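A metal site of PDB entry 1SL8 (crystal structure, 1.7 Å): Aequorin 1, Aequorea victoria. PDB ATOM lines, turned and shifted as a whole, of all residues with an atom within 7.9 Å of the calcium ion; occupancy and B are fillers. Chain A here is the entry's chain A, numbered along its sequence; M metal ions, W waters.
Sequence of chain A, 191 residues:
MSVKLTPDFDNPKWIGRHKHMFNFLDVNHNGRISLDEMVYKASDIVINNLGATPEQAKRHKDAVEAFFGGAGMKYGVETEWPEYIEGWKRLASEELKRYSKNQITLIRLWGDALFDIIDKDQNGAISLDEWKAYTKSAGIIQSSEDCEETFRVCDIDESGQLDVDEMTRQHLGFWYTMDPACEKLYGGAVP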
ATOM      1  N   ALA A 125       4.330 -14.484 -23.784  1.00  0.00           N
ATOM      2  CA  ALA A 125       5.163 -15.198 -22.796  1.00  0.00           C
ATOM      3  C   ALA A 125       6.197 -14.203 -22.285  1.00  0.00           C
ATOM      4  O   ALA A 125       6.562 -13.253 -22.989  1.00  0.00           O
ATOM      5  CB  ALA A 125       5.826 -16.345 -23.410  1.00  0.00           C
ATOM      6  N   ILE A 126       6.642 -14.400 -21.048  1.00  0.00           N
ATOM      7  CA  ILE A 126       7.592 -13.425 -20.474  1.00  0.00           C
ATOM      8  C   ILE A 126       8.974 -13.983 -20.575  1.00  0.00           C
ATOM      9  O   ILE A 126       9.280 -15.011 -19.964  1.00  0.00           O
ATOM     10  CB  ILE A 126       7.219 -13.154 -18.963  1.00  0.00           C
ATOM     11  CG1 ILE A 126       5.705 -12.791 -18.822  1.00  0.00           C
ATOM     12  CG2 ILE A 126       8.186 -12.088 -18.357  1.00  0.00           C
ATOM     13  CD1 ILE A 126       5.121 -11.618 -19.624  1.00  0.00           C
ATOM     14  N   PHE A 151      13.219 -16.263 -11.617  1.00  0.00           N
ATOM     15  CA  PHE A 151      12.673 -16.666 -12.936  1.00  0.00           C
ATOM     16  C   PHE A 151      12.558 -18.196 -13.012  1.00  0.00           C
ATOM     17  O   PHE A 151      11.454 -18.678 -13.383  1.00  0.00           O
ATOM     18  CB  PHE A 151      13.587 -16.136 -14.053  1.00  0.00           C
ATOM     19  CG  PHE A 151      13.043 -16.369 -15.422  1.00  0.00           C
ATOM     20  CD1 PHE A 151      12.199 -15.455 -16.020  1.00  0.00           C
ATOM     21  CD2 PHE A 151      13.375 -17.530 -16.092  1.00  0.00           C
ATOM     22  CE1 PHE A 151      11.668 -15.682 -17.332  1.00  0.00           C
ATOM     23  CE2 PHE A 151      12.849 -17.745 -17.444  1.00  0.00           C
ATOM     24  CZ  PHE A 151      12.034 -16.856 -18.004  1.00  0.00           C
ATOM     25  N   CYS A 154       9.647 -19.451 -11.064  1.00  0.00           N
ATOM     26  CA  CYS A 154       8.406 -19.152 -11.739  1.00  0.00           C
ATOM     27  C   CYS A 154       8.149 -20.092 -12.933  1.00  0.00           C
ATOM     28  O   CYS A 154       6.997 -20.485 -13.170  1.00  0.00           O
ATOM     29  CB  CYS A 154       8.364 -17.702 -12.255  1.00  0.00           C
ATOM     30  SG  CYS A 154       6.702 -17.232 -12.748  1.00  0.00           S
ATOM     31  N   ASP A 155       9.234 -20.470 -13.567  1.00  0.00           N
ATOM     32  CA  ASP A 155       9.148 -21.184 -14.884  1.00  0.00           C
ATOM     33  C   ASP A 155       8.992 -22.695 -14.657  1.00  0.00           C
ATOM     34  O   ASP A 155       9.873 -23.499 -14.911  1.00  0.00           O
ATOM     35  CB  ASP A 155      10.387 -20.799 -15.706  1.00  0.00           C
ATOM     36  CG  ASP A 155      10.349 -21.403 -17.114  1.00  0.00           C
ATOM     37  OD1 ASP A 155       9.190 -21.631 -17.584  1.00  0.00           O
ATOM     38  OD2 ASP A 155      11.387 -21.613 -17.755  1.00  0.00           O
ATOM     39  N   ILE A 156       7.802 -23.071 -14.205  1.00  0.00           N
ATOM     40  CA  ILE A 156       7.560 -24.443 -13.742  1.00  0.00           C
ATOM     41  C   ILE A 156       7.916 -25.542 -14.784  1.00  0.00           C
ATOM     42  O   ILE A 156       8.433 -26.605 -14.460  1.00  0.00           O
ATOM     43  CB  ILE A 156       6.045 -24.590 -13.337  1.00  0.00           C
ATOM     44  CG1 ILE A 156       5.654 -23.548 -12.271  1.00  0.00           C
ATOM     45  CG2 ILE A 156       5.773 -25.999 -12.841  1.00  0.00           C
ATOM     46  CD1 ILE A 156       6.421 -23.700 -11.018  1.00  0.00           C
ATOM     47  N   ASP A 157       7.571 -25.298 -16.040  1.00  0.00           N
ATOM     48  CA  ASP A 157       7.859 -26.338 -17.072  1.00  0.00           C
ATOM     49  C   ASP A 157       9.212 -26.175 -17.700  1.00  0.00           C
ATOM     50  O   ASP A 157       9.551 -26.896 -18.693  1.00  0.00           O
ATOM     51  CB  ASP A 157       6.733 -26.280 -18.167  1.00  0.00           C
ATOM     52  CG  ASP A 157       6.715 -24.980 -18.992  1.00  0.00           C
ATOM     53  OD1 ASP A 157       7.448 -23.972 -18.781  1.00  0.00           O
ATOM     54  OD2 ASP A 157       5.863 -24.867 -19.919  1.00  0.00           O
ATOM     55  N   GLU A 158       9.986 -25.218 -17.191  1.00  0.00           N
ATOM     56  CA  GLU A 158      11.333 -24.919 -17.645  1.00  0.00           C
ATOM     57  C   GLU A 158      11.384 -24.698 -19.150  1.00  0.00           C
ATOM     58  O   GLU A 158      12.358 -25.088 -19.791  1.00  0.00           O
ATOM     59  CB  GLU A 158      12.319 -26.060 -17.293  1.00  0.00           C
ATOM     60  CG  GLU A 158      12.555 -26.306 -15.766  1.00  0.00           C
ATOM     61  CD  GLU A 158      13.821 -27.096 -15.564  1.00  0.00           C
ATOM     62  OE1 GLU A 158      14.892 -26.484 -15.336  1.00  0.00           O
ATOM     63  OE2 GLU A 158      13.806 -28.327 -15.734  1.00  0.00           O
ATOM     64  N   SER A 159      10.356 -24.082 -19.671  1.00  0.00           N
ATOM     65  CA  SER A 159      10.276 -23.747 -21.102  1.00  0.00           C
ATOM     66  C   SER A 159      11.234 -22.619 -21.489  1.00  0.00           C
ATOM     67  O   SER A 159      11.565 -22.449 -22.699  1.00  0.00           O
ATOM     68  CB  SER A 159       8.815 -23.371 -21.444  1.00  0.00           C
ATOM     69  OG  SER A 159       8.427 -22.054 -21.014  1.00  0.00           O
ATOM     70  N   GLY A 160      11.713 -21.853 -20.496  1.00  0.00           N
ATOM     71  CA  GLY A 160      12.533 -20.689 -20.757  1.00  0.00           C
ATOM     72  C   GLY A 160      11.801 -19.359 -20.834  1.00  0.00           C
ATOM     73  O   GLY A 160      12.449 -18.327 -20.913  1.00  0.00           O
ATOM     74  N   GLN A 161      10.461 -19.398 -20.842  1.00  0.00           N
ATOM     75  CA  GLN A 161       9.616 -18.222 -20.736  1.00  0.00           C
ATOM     76  C   GLN A 161       8.413 -18.464 -19.860  1.00  0.00           C
ATOM     77  O   GLN A 161       8.003 -19.609 -19.623  1.00  0.00           O
ATOM     78  CB  GLN A 161       9.069 -17.793 -22.097  1.00  0.00           C
ATOM     79  CG  GLN A 161      10.148 -17.340 -23.046  1.00  0.00           C
ATOM     80  CD  GLN A 161       9.490 -16.631 -24.265  1.00  0.00           C
ATOM     81  OE1 GLN A 161       9.169 -15.449 -24.236  1.00  0.00           O
ATOM     82  NE2 GLN A 161       9.232 -17.420 -25.313  1.00  0.00           N
ATOM     83  N   LEU A 162       7.864 -17.342 -19.361  1.00  0.00           N
ATOM     84  CA  LEU A 162       6.778 -17.496 -18.382  1.00  0.00           C
ATOM     85  C   LEU A 162       5.442 -17.261 -19.026  1.00  0.00           C
ATOM     86  O   LEU A 162       5.173 -16.168 -19.589  1.00  0.00           O
ATOM     87  CB  LEU A 162       6.939 -16.607 -17.116  1.00  0.00           C
ATOM     88  CG  LEU A 162       8.370 -16.530 -16.593  1.00  0.00           C
ATOM     89  CD1 LEU A 162       8.390 -15.412 -15.421  1.00  0.00           C
ATOM     90  CD2 LEU A 162       8.867 -17.819 -16.062  1.00  0.00           C
ATOM     91  N   ASP A 163       4.586 -18.289 -18.939  1.00  0.00           N
ATOM     92  CA  ASP A 163       3.219 -18.137 -19.425  1.00  0.00           C
ATOM     93  C   ASP A 163       2.233 -17.480 -18.451  1.00  0.00           C
ATOM     94  O   ASP A 163       2.569 -17.176 -17.278  1.00  0.00           O
ATOM     95  CB  ASP A 163       2.678 -19.435 -20.040  1.00  0.00           C
ATOM     96  CG  ASP A 163       2.534 -20.567 -19.062  1.00  0.00           C
ATOM     97  OD1 ASP A 163       2.145 -20.348 -17.905  1.00  0.00           O
ATOM     98  OD2 ASP A 163       2.765 -21.740 -19.377  1.00  0.00           O
ATOM     99  N   VAL A 164       1.000 -17.209 -18.925  1.00  0.00           N
ATOM    100  CA  VAL A 164      -0.012 -16.601 -18.085  1.00  0.00           C
ATOM    101  C   VAL A 164      -0.270 -17.403 -16.803  1.00  0.00           C
ATOM    102  O   VAL A 164      -0.391 -16.779 -15.730  1.00  0.00           O
ATOM    103  CB  VAL A 164      -1.345 -16.369 -18.868  1.00  0.00           C
ATOM    104  CG1 VAL A 164      -2.424 -15.838 -17.939  1.00  0.00           C
ATOM    105  CG2 VAL A 164      -1.135 -15.362 -20.013  1.00  0.00           C
ATOM    106  N   GLU A 166       1.767 -19.591 -15.232  1.00  0.00           N
ATOM    107  CA  GLU A 166       2.960 -19.410 -14.370  1.00  0.00           C
ATOM    108  C   GLU A 166       2.966 -18.070 -13.663  1.00  0.00           C
ATOM    109  O   GLU A 166       3.269 -17.980 -12.457  1.00  0.00           O
ATOM    110  CB  GLU A 166       4.296 -19.627 -15.120  1.00  0.00           C
ATOM    111  CG  GLU A 166       4.433 -21.087 -15.528  1.00  0.00           C
ATOM    112  CD  GLU A 166       5.430 -21.322 -16.665  1.00  0.00           C
ATOM    113  OE1 GLU A 166       5.789 -20.347 -17.354  1.00  0.00           O
ATOM    114  OE2 GLU A 166       5.919 -22.447 -16.766  1.00  0.00           O
ATOM    115  N   ARG A 169       0.297 -18.065 -10.890  1.00  0.00           N
ATOM    116  CA  ARG A 169       0.754 -18.767  -9.686  1.00  0.00           C
ATOM    117  C   ARG A 169       1.728 -17.881  -8.922  1.00  0.00           C
ATOM    118  O   ARG A 169       1.748 -17.888  -7.687  1.00  0.00           O
ATOM    119  CB  ARG A 169       1.399 -20.104 -10.074  1.00  0.00           C
ATOM    120  CG  ARG A 169       0.358 -21.098 -10.526  1.00  0.00           C
ATOM    121  CD  ARG A 169       0.890 -22.522 -10.766  1.00  0.00           C
ATOM    122  NE  ARG A 169       1.302 -22.684 -12.161  1.00  0.00           N
ATOM    123  CZ  ARG A 169       1.639 -23.851 -12.755  1.00  0.00           C
ATOM    124  NH1 ARG A 169       1.620 -25.003 -12.064  1.00  0.00           N
ATOM    125  NH2 ARG A 169       2.003 -23.854 -14.060  1.00  0.00           N
HETATM  126 CA    CA M   1       7.289 -21.736 -18.849  1.00  0.00          CA
HETATM  127  O   HOH W   1       5.412 -22.137 -20.202  1.00  0.00           O
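The backbone NH (N) of Ile 156 lies close to the side-chain carboxylate (OE2) of Glu 166 (3.2 Å).
N of Glu 166 sits at hydrogen-bond distance from OD1 of Asp 163, 2.8 Å away.
SG of Cys 154 lies within hydrogen-bond range of O of Glu 166 (3.5 Å).
The side-chain carboxylate (OD2) of Asp 155 lies within hydrogen-bond range of the backbone NH (N) of Gly 160 (2.8 Å).
Of the 16 residues printed, 5 come within 4 Å of the calcium ion.
The calcium ion is bound by OD1 of Asp 157 (2.2 Å), OD1 of Asp 155 (2.3 Å), water W1 (2.3 Å), O of Gln 161 (2.4 Å), OG of Ser 159 (2.5 Å), OE1 of Glu 166 (2.5 Å) and OE2 of Glu 166 (2.6 Å).
The calcium ion has seven donor atoms within binding distance.
Water W1 bridges OD2 of Asp 157 (2.8 Å) and OD2 of Asp 163 (2.8 Å).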
